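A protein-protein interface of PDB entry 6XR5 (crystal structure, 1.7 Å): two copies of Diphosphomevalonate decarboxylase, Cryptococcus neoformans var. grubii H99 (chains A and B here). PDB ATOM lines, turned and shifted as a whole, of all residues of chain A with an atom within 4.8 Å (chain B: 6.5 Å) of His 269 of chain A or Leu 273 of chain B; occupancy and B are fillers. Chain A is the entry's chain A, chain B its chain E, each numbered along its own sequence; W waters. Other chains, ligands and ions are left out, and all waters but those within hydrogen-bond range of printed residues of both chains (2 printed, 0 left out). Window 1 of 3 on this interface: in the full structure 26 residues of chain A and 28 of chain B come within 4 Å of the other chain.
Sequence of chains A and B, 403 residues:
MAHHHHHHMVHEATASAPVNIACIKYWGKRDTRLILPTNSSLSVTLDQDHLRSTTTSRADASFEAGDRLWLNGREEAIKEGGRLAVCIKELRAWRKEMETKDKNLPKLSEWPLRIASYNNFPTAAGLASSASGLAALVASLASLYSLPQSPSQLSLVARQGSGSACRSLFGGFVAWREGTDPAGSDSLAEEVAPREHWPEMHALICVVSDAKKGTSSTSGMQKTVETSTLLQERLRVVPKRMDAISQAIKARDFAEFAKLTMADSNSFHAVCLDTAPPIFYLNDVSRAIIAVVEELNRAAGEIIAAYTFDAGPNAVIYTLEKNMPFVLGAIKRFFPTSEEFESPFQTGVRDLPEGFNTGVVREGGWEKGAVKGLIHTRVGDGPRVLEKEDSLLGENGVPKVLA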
ATOM      1  N   SER A 265      -0.193  21.183 -10.223  1.00  0.00           N
ATOM      2  CA  SER A 265      -1.479  21.782  -9.868  1.00  0.00           C
ATOM      3  C   SER A 265      -1.724  21.654  -8.370  1.00  0.00           C
ATOM      4  O   SER A 265      -2.063  22.631  -7.688  1.00  0.00           O
ATOM      5  CB  SER A 265      -2.611  21.087 -10.645  1.00  0.00           C
ATOM      6  OG  SER A 265      -3.861  21.706 -10.339  1.00  0.00           O
ATOM      7  N   ASN A 266      -1.569  20.447  -7.836  1.00  0.00           N
ATOM      8  CA  ASN A 266      -1.805  20.264  -6.398  1.00  0.00           C
ATOM      9  C   ASN A 266      -0.810  21.077  -5.563  1.00  0.00           C
ATOM     10  O   ASN A 266      -1.161  21.636  -4.505  1.00  0.00           O
ATOM     11  CB  ASN A 266      -1.732  18.771  -6.079  1.00  0.00           C
ATOM     12  CG  ASN A 266      -2.839  17.973  -6.746  1.00  0.00           C
ATOM     13  OD1 ASN A 266      -3.935  18.491  -7.023  1.00  0.00           O
ATOM     14  ND2 ASN A 266      -2.559  16.670  -7.017  1.00  0.00           N
ATOM     15  N   SER A 267       0.436  21.187  -6.050  1.00  0.00           N
ATOM     16  CA  SER A 267       1.453  21.967  -5.348  1.00  0.00           C
ATOM     17  C   SER A 267       1.040  23.434  -5.247  1.00  0.00           C
ATOM     18  O   SER A 267       1.169  24.065  -4.180  1.00  0.00           O
ATOM     19  CB  SER A 267       2.788  21.830  -6.093  1.00  0.00           C
ATOM     20  OG  SER A 267       3.794  22.615  -5.472  1.00  0.00           O
ATOM     21  N   PHE A 268       0.489  23.971  -6.330  1.00  0.00           N
ATOM     22  CA  PHE A 268       0.015  25.350  -6.329  1.00  0.00           C
ATOM     23  C   PHE A 268      -1.143  25.529  -5.349  1.00  0.00           C
ATOM     24  O   PHE A 268      -1.135  26.457  -4.514  1.00  0.00           O
ATOM     25  CB  PHE A 268      -0.357  25.714  -7.779  1.00  0.00           C
ATOM     26  CG  PHE A 268      -1.358  26.825  -7.907  1.00  0.00           C
ATOM     27  CD1 PHE A 268      -1.148  28.085  -7.315  1.00  0.00           C
ATOM     28  CD2 PHE A 268      -2.514  26.622  -8.658  1.00  0.00           C
ATOM     29  CE1 PHE A 268      -2.080  29.077  -7.440  1.00  0.00           C
ATOM     30  CE2 PHE A 268      -3.462  27.633  -8.794  1.00  0.00           C
ATOM     31  CZ  PHE A 268      -3.246  28.887  -8.180  1.00  0.00           C
ATOM     32  N   HIS A 269      -2.131  24.625  -5.386  1.00  0.00           N
ATOM     33  CA  HIS A 269      -3.230  24.782  -4.432  1.00  0.00           C
ATOM     34  C   HIS A 269      -2.779  24.509  -3.014  1.00  0.00           C
ATOM     35  O   HIS A 269      -3.302  25.137  -2.066  1.00  0.00           O
ATOM     36  CB  HIS A 269      -4.420  23.926  -4.872  1.00  0.00           C
ATOM     37  CG  HIS A 269      -5.025  24.450  -6.137  1.00  0.00           C
ATOM     38  ND1 HIS A 269      -5.912  25.513  -6.136  1.00  0.00           N
ATOM     39  CD2 HIS A 269      -4.746  24.188  -7.440  1.00  0.00           C
ATOM     40  CE1 HIS A 269      -6.197  25.841  -7.391  1.00  0.00           C
ATOM     41  NE2 HIS A 269      -5.509  25.049  -8.199  1.00  0.00           N
ATOM     42  N   ALA A 270      -1.720  23.725  -2.846  1.00  0.00           N
ATOM     43  CA  ALA A 270      -1.176  23.538  -1.501  1.00  0.00           C
ATOM     44  C   ALA A 270      -0.564  24.830  -0.954  1.00  0.00           C
ATOM     45  O   ALA A 270      -0.767  25.164   0.217  1.00  0.00           O
ATOM     46  CB  ALA A 270      -0.157  22.396  -1.495  1.00  0.00           C
ATOM     47  N   VAL A 271       0.240  25.547  -1.752  1.00  0.00           N
ATOM     48  CA  VAL A 271       0.821  26.772  -1.171  1.00  0.00           C
ATOM     49  C   VAL A 271      -0.235  27.858  -0.992  1.00  0.00           C
ATOM     50  O   VAL A 271      -0.079  28.736  -0.117  1.00  0.00           O
ATOM     51  CB  VAL A 271       2.026  27.267  -2.012  1.00  0.00           C
ATOM     52  CG1 VAL A 271       3.153  26.205  -2.036  1.00  0.00           C
ATOM     53  CG2 VAL A 271       1.634  27.717  -3.475  1.00  0.00           C
ATOM     54  N   CYS A 272      -1.321  27.822  -1.783  1.00  0.00           N
ATOM     55  CA  CYS A 272      -2.448  28.704  -1.491  1.00  0.00           C
ATOM     56  C   CYS A 272      -3.042  28.387  -0.124  1.00  0.00           C
ATOM     57  O   CYS A 272      -3.327  29.289   0.661  1.00  0.00           O
ATOM     58  CB  CYS A 272      -3.536  28.581  -2.564  1.00  0.00           C
ATOM     59  SG  CYS A 272      -3.080  29.332  -4.150  1.00  0.00           S
ATOM     60  N   LEU A 273      -3.221  27.107   0.183  1.00  0.00           N
ATOM     61  CA  LEU A 273      -3.758  26.753   1.494  1.00  0.00           C
ATOM     62  C   LEU A 273      -2.820  27.164   2.618  1.00  0.00           C
ATOM     63  O   LEU A 273      -3.275  27.476   3.720  1.00  0.00           O
ATOM     64  CB  LEU A 273      -4.024  25.241   1.526  1.00  0.00           C
ATOM     65  CG  LEU A 273      -4.807  24.543   2.639  1.00  0.00           C
ATOM     66  CD1 LEU A 273      -5.849  25.367   3.361  1.00  0.00           C
ATOM     67  CD2 LEU A 273      -5.423  23.197   2.128  1.00  0.00           C
ATOM     68  N   TYR A 281      -9.408  27.896  -3.827  1.00  0.00           N
ATOM     69  CA  TYR A 281      -9.925  27.925  -5.193  1.00  0.00           C
ATOM     70  C   TYR A 281     -10.682  26.659  -5.557  1.00  0.00           C
ATOM     71  O   TYR A 281     -11.764  26.734  -6.168  1.00  0.00           O
ATOM     72  CB  TYR A 281      -8.770  28.102  -6.192  1.00  0.00           C
ATOM     73  CG  TYR A 281      -8.170  29.494  -6.124  1.00  0.00           C
ATOM     74  CD1 TYR A 281      -8.974  30.606  -6.218  1.00  0.00           C
ATOM     75  CD2 TYR A 281      -6.784  29.668  -6.007  1.00  0.00           C
ATOM     76  CE1 TYR A 281      -8.415  31.874  -6.189  1.00  0.00           C
ATOM     77  CE2 TYR A 281      -6.227  30.938  -5.989  1.00  0.00           C
ATOM     78  CZ  TYR A 281      -7.045  32.019  -6.074  1.00  0.00           C
ATOM     79  OH  TYR A 281      -6.488  33.281  -6.030  1.00  0.00           O
ATOM     80  N   LEU A 282     -10.151  25.502  -5.193  1.00  0.00           N
ATOM     81  CA  LEU A 282     -10.880  24.263  -5.418  1.00  0.00           C
ATOM     82  C   LEU A 282     -12.137  24.255  -4.566  1.00  0.00           C
ATOM     83  O   LEU A 282     -12.127  24.715  -3.420  1.00  0.00           O
ATOM     84  CB  LEU A 282     -10.030  23.045  -5.038  1.00  0.00           C
ATOM     85  CG  LEU A 282      -8.648  22.949  -5.657  1.00  0.00           C
ATOM     86  CD1 LEU A 282      -7.977  21.693  -5.127  1.00  0.00           C
ATOM     87  CD2 LEU A 282      -8.716  22.931  -7.200  1.00  0.00           C
ATOM     88  N   PHE A 309      -5.848  22.889 -12.287  1.00  0.00           N
ATOM     89  CA  PHE A 309      -6.789  23.916 -11.867  1.00  0.00           C
ATOM     90  C   PHE A 309      -6.017  25.201 -11.721  1.00  0.00           C
ATOM     91  O   PHE A 309      -4.930  25.211 -11.135  1.00  0.00           O
ATOM     92  CB  PHE A 309      -7.437  23.560 -10.523  1.00  0.00           C
ATOM     93  CG  PHE A 309      -8.324  22.341 -10.572  1.00  0.00           C
ATOM     94  CD1 PHE A 309      -7.799  21.049 -10.549  1.00  0.00           C
ATOM     95  CD2 PHE A 309      -9.706  22.511 -10.672  1.00  0.00           C
ATOM     96  CE1 PHE A 309      -8.628  19.934 -10.603  1.00  0.00           C
ATOM     97  CE2 PHE A 309     -10.551  21.396 -10.712  1.00  0.00           C
ATOM     98  CZ  PHE A 309     -10.008  20.113 -10.668  1.00  0.00           C
ATOM     99  N   ASP A 310      -6.570  26.272 -12.280  1.00  0.00           N
ATOM    100  CA  ASP A 310      -5.973  27.586 -12.064  1.00  0.00           C
ATOM    101  C   ASP A 310      -6.631  28.254 -10.860  1.00  0.00           C
ATOM    102  O   ASP A 310      -6.921  27.575  -9.872  1.00  0.00           O
ATOM    103  CB  ASP A 310      -6.104  28.421 -13.322  1.00  0.00           C
ATOM    104  CG  ASP A 310      -5.071  28.034 -14.384  1.00  0.00           C
ATOM    105  OD1 ASP A 310      -3.960  27.584 -14.008  1.00  0.00           O
ATOM    106  OD2 ASP A 310      -5.356  28.245 -15.582  1.00  0.00           O
ATOM    107  N   GLY A 312      -9.402  29.129  -9.507  1.00  0.00           N
ATOM    108  CA  GLY A 312     -10.824  28.957  -9.371  1.00  0.00           C
ATOM    109  C   GLY A 312     -11.101  27.473  -9.486  1.00  0.00           C
ATOM    110  O   GLY A 312     -10.184  26.675  -9.659  1.00  0.00           O
ATOM    111  N   PHE B 268      -0.746  21.418   7.553  1.00  0.00           N
ATOM    112  CA  PHE B 268      -1.115  19.997   7.481  1.00  0.00           C
ATOM    113  C   PHE B 268      -2.008  19.722   6.268  1.00  0.00           C
ATOM    114  O   PHE B 268      -1.737  18.814   5.461  1.00  0.00           O
ATOM    115  CB  PHE B 268      -1.787  19.621   8.819  1.00  0.00           C
ATOM    116  CG  PHE B 268      -2.637  18.409   8.758  1.00  0.00           C
ATOM    117  CD1 PHE B 268      -2.136  17.242   8.223  1.00  0.00           C
ATOM    118  CD2 PHE B 268      -3.916  18.423   9.282  1.00  0.00           C
ATOM    119  CE1 PHE B 268      -2.905  16.085   8.163  1.00  0.00           C
ATOM    120  CE2 PHE B 268      -4.718  17.277   9.239  1.00  0.00           C
ATOM    121  CZ  PHE B 268      -4.211  16.093   8.682  1.00  0.00           C
ATOM    122  N   HIS B 269      -3.062  20.517   6.092  1.00  0.00           N
ATOM    123  CA  HIS B 269      -3.932  20.268   4.947  1.00  0.00           C
ATOM    124  C   HIS B 269      -3.235  20.575   3.634  1.00  0.00           C
ATOM    125  O   HIS B 269      -3.531  19.928   2.612  1.00  0.00           O
ATOM    126  CB  HIS B 269      -5.254  21.016   5.150  1.00  0.00           C
ATOM    127  CG  HIS B 269      -6.057  20.395   6.258  1.00  0.00           C
ATOM    128  ND1 HIS B 269      -6.755  19.219   6.072  1.00  0.00           N
ATOM    129  CD2 HIS B 269      -6.106  20.648   7.590  1.00  0.00           C
ATOM    130  CE1 HIS B 269      -7.266  18.818   7.222  1.00  0.00           C
ATOM    131  NE2 HIS B 269      -6.900  19.675   8.159  1.00  0.00           N
ATOM    132  N   ALA B 270      -2.263  21.488   3.644  1.00  0.00           N
ATOM    133  CA  ALA B 270      -1.479  21.737   2.432  1.00  0.00           C
ATOM    134  C   ALA B 270      -0.656  20.504   2.036  1.00  0.00           C
ATOM    135  O   ALA B 270      -0.611  20.136   0.850  1.00  0.00           O
ATOM    136  CB  ALA B 270      -0.579  22.961   2.632  1.00  0.00           C
ATOM    137  N   VAL B 271       0.037  19.872   2.999  1.00  0.00           N
ATOM    138  CA  VAL B 271       0.844  18.715   2.583  1.00  0.00           C
ATOM    139  C   VAL B 271      -0.033  17.542   2.206  1.00  0.00           C
ATOM    140  O   VAL B 271       0.368  16.730   1.354  1.00  0.00           O
ATOM    141  CB  VAL B 271       1.911  18.328   3.633  1.00  0.00           C
ATOM    142  CG1 VAL B 271       2.883  19.532   3.848  1.00  0.00           C
ATOM    143  CG2 VAL B 271       1.293  17.831   4.970  1.00  0.00           C
ATOM    144  N   CYS B 272      -1.256  17.469   2.744  1.00  0.00           N
ATOM    145  CA  CYS B 272      -2.208  16.481   2.233  1.00  0.00           C
ATOM    146  C   CYS B 272      -2.546  16.771   0.781  1.00  0.00           C
ATOM    147  O   CYS B 272      -2.607  15.859  -0.041  1.00  0.00           O
ATOM    148  CB  CYS B 272      -3.498  16.467   3.063  1.00  0.00           C
ATOM    149  SG  CYS B 272      -3.315  15.744   4.717  1.00  0.00           S
ATOM    150  N   LEU B 273      -2.802  18.038   0.452  1.00  0.00           N
ATOM    151  CA  LEU B 273      -3.097  18.377  -0.937  1.00  0.00           C
ATOM    152  C   LEU B 273      -1.918  18.064  -1.844  1.00  0.00           C
ATOM    153  O   LEU B 273      -2.111  17.658  -2.999  1.00  0.00           O
ATOM    154  CB  LEU B 273      -3.457  19.875  -1.041  1.00  0.00           C
ATOM    155  CG  LEU B 273      -4.682  20.247  -1.890  1.00  0.00           C
ATOM    156  CD1 LEU B 273      -5.011  21.770  -1.772  1.00  0.00           C
ATOM    157  CD2 LEU B 273      -4.468  19.887  -3.346  1.00  0.00           C
ATOM    158  N   ASP B 274      -0.703  18.194  -1.335  1.00  0.00           N
ATOM    159  CA  ASP B 274       0.519  17.974  -2.120  1.00  0.00           C
ATOM    160  C   ASP B 274       0.910  16.498  -2.220  1.00  0.00           C
ATOM    161  O   ASP B 274       1.918  16.191  -2.854  1.00  0.00           O
ATOM    162  CB  ASP B 274       1.680  18.761  -1.487  1.00  0.00           C
ATOM    163  CG  ASP B 274       2.964  18.731  -2.311  1.00  0.00           C
ATOM    164  OD1 ASP B 274       2.939  19.166  -3.488  1.00  0.00           O
ATOM    165  OD2 ASP B 274       4.019  18.335  -1.740  1.00  0.00           O
ATOM    166  N   THR B 275       0.157  15.614  -1.588  1.00  0.00           N
ATOM    167  CA  THR B 275       0.370  14.174  -1.716  1.00  0.00           C
ATOM    168  C   THR B 275      -0.067  13.735  -3.112  1.00  0.00           C
ATOM    169  O   THR B 275      -0.906  14.381  -3.745  1.00  0.00           O
ATOM    170  CB  THR B 275      -0.410  13.476  -0.610  1.00  0.00           C
ATOM    171  OG1 THR B 275       0.066  13.999   0.653  1.00  0.00           O
ATOM    172  CG2 THR B 275      -0.249  11.934  -0.631  1.00  0.00           C
ATOM    173  N   ALA B 276       0.500  12.620  -3.584  1.00  0.00           N
ATOM    174  CA  ALA B 276       0.158  12.080  -4.894  1.00  0.00           C
ATOM    175  C   ALA B 276      -0.282  10.635  -4.706  1.00  0.00           C
ATOM    176  O   ALA B 276       0.564   9.785  -4.374  1.00  0.00           O
ATOM    177  CB  ALA B 276       1.341  12.161  -5.853  1.00  0.00           C
ATOM    178  N   PRO B 277      -1.581  10.310  -4.846  1.00  0.00           N
ATOM    179  CA  PRO B 277      -2.708  11.211  -5.151  1.00  0.00           C
ATOM    180  C   PRO B 277      -3.028  12.153  -3.979  1.00  0.00           C
ATOM    181  O   PRO B 277      -2.738  11.809  -2.828  1.00  0.00           O
ATOM    182  CB  PRO B 277      -3.879  10.254  -5.365  1.00  0.00           C
ATOM    183  CG  PRO B 277      -3.279   8.900  -5.482  1.00  0.00           C
ATOM    184  CD  PRO B 277      -2.049   8.927  -4.664  1.00  0.00           C
ATOM    185  N   PRO B 278      -3.652  13.297  -4.237  1.00  0.00           N
ATOM    186  CA  PRO B 278      -3.926  14.236  -3.136  1.00  0.00           C
ATOM    187  C   PRO B 278      -4.943  13.693  -2.140  1.00  0.00           C
ATOM    188  O   PRO B 278      -5.819  12.888  -2.467  1.00  0.00           O
ATOM    189  CB  PRO B 278      -4.462  15.489  -3.850  1.00  0.00           C
ATOM    190  CG  PRO B 278      -5.035  14.963  -5.142  1.00  0.00           C
ATOM    191  CD  PRO B 278      -4.154  13.790  -5.532  1.00  0.00           C
ATOM    192  N   ILE B 279      -4.801  14.158  -0.903  1.00  0.00           N
ATOM    193  CA  ILE B 279      -5.675  13.816   0.211  1.00  0.00           C
ATOM    194  C   ILE B 279      -6.465  15.059   0.582  1.00  0.00           C
ATOM    195  O   ILE B 279      -5.881  16.134   0.749  1.00  0.00           O
ATOM    196  CB  ILE B 279      -4.866  13.310   1.417  1.00  0.00           C
ATOM    197  CG1 ILE B 279      -4.179  11.989   1.084  1.00  0.00           C
ATOM    198  CG2 ILE B 279      -5.796  13.128   2.608  1.00  0.00           C
ATOM    199  CD1 ILE B 279      -3.109  11.628   2.124  1.00  0.00           C
ATOM    200  N   PHE B 280      -7.793  14.925   0.650  1.00  0.00           N
ATOM    201  CA  PHE B 280      -8.680  16.055   0.918  1.00  0.00           C
ATOM    202  C   PHE B 280      -9.507  15.737   2.152  1.00  0.00           C
ATOM    203  O   PHE B 280     -10.236  14.747   2.168  1.00  0.00           O
ATOM    204  CB  PHE B 280      -9.626  16.351  -0.257  1.00  0.00           C
ATOM    205  CG  PHE B 280      -8.925  16.705  -1.552  1.00  0.00           C
ATOM    206  CD1 PHE B 280      -8.340  17.947  -1.724  1.00  0.00           C
ATOM    207  CD2 PHE B 280      -8.901  15.802  -2.604  1.00  0.00           C
ATOM    208  CE1 PHE B 280      -7.699  18.285  -2.940  1.00  0.00           C
ATOM    209  CE2 PHE B 280      -8.274  16.126  -3.808  1.00  0.00           C
ATOM    210  CZ  PHE B 280      -7.676  17.357  -3.980  1.00  0.00           C
HETATM  211  O   HOH W   1       0.044  15.690  -5.951  1.00  0.00           O
HETATM  212  O   HOH W   2       5.051  20.425  -4.544  1.00  0.00           O
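His 269 of chain A touches Leu 273 of chain B, and with the chains exchanged Leu 273 of chain A touches His 269 of chain B.
Ala 270 of chain B touches its own counterpart, Ala 270 of chain A.
Ala 270 of chain A touches Leu 273 of chain B, and with the chains exchanged Leu 273 of chain A touches Ala 270 of chain B.
6 positions are printed for both chains.
Of the 8 pairs that touch across the chains among the printed residues, 5 have their exchanged pair printed and touching as well.
Water W2 bridges the side-chain carboxylate of Asp 274 of chain B (2.7 Å) and the side-chain hydroxyl of Ser 267 of chain A (2.7 Å).
Water W1 lies within hydrogen-bond range of O of Thr 275 of chain B (2.7 Å) and ND2 of Asn 266 of chain A (3.0 Å).
His 269 of chain A touches one residue of chain B.
Leu 273 of chain B touches three residues of chain A.
Of the printed residues of chain B, Ala 270 of chain A touches Ala 270 and Leu 273.
Printed residues of chain A within 4 Å of Pro 278 of chain B: Asn 266 (3.5 Å).
Of the printed residues of chain B, Ser 267 of chain A touches Asp 274.
Printed residues of chain A within 4 Å of Ala 270 of chain B: Ala 270 and Leu 273.
Printed residues of chain A within 4 Å of Asp 274 of chain B: Ser 267.
Ser 265 of chain A touches none of the printed residues of chain B.
The nearest residue of chain B that does not touch His 269 of chain A is Ala 270 of chain B (5.8 Å).
CB of Asn 266 of chain A touches O of Leu 273 of chain B, at 3.3 Å.
Asn 266 of chain A touches Pro 278 of chain B (ND2 to CG, 3.5 Å).
OD1 of Asp 274 of chain B touches CA of Ser 267 of chain A (3.7 Å).
C of His 269 of chain A touches CD1 of Leu 273 of chain B, at 3.7 Å.
CB of Ala 270 of chain B touches O of Ala 270 of chain A, at 3.3 Å.
Ala 270 of chain A touches Leu 273 of chain B (N to CD1, 3.98 Å).
CB of His 269 of chain B touches CD2 of Leu 273 of chain A, 3.7 Å away.
Leu 273 of chain A touches Ala 270 of chain B (CD2 to N, 3.9 Å).
Hydrophobic or aromatic side chains of chain A within 4 Å of the printed part of chain B: His 269, Ala 270 and Leu 273.
Of the 13 printed residues of chain B, 5 touch a printed residue of chain A.
Among the printed residues, 8 pairs touch across the chains.
Among the printed residues, no Asp or Glu carboxylate lies within 4 Å of a Lys or Arg side-chain nitrogen of the other chain.
NE2 of His 269 of chain A lies within hydrogen-bond range of O of Phe 309 of chain A, at 3.0 Å.
O of Asp 310 of chain A sits close to NE2 of His 269 of chain A (3.3 Å).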
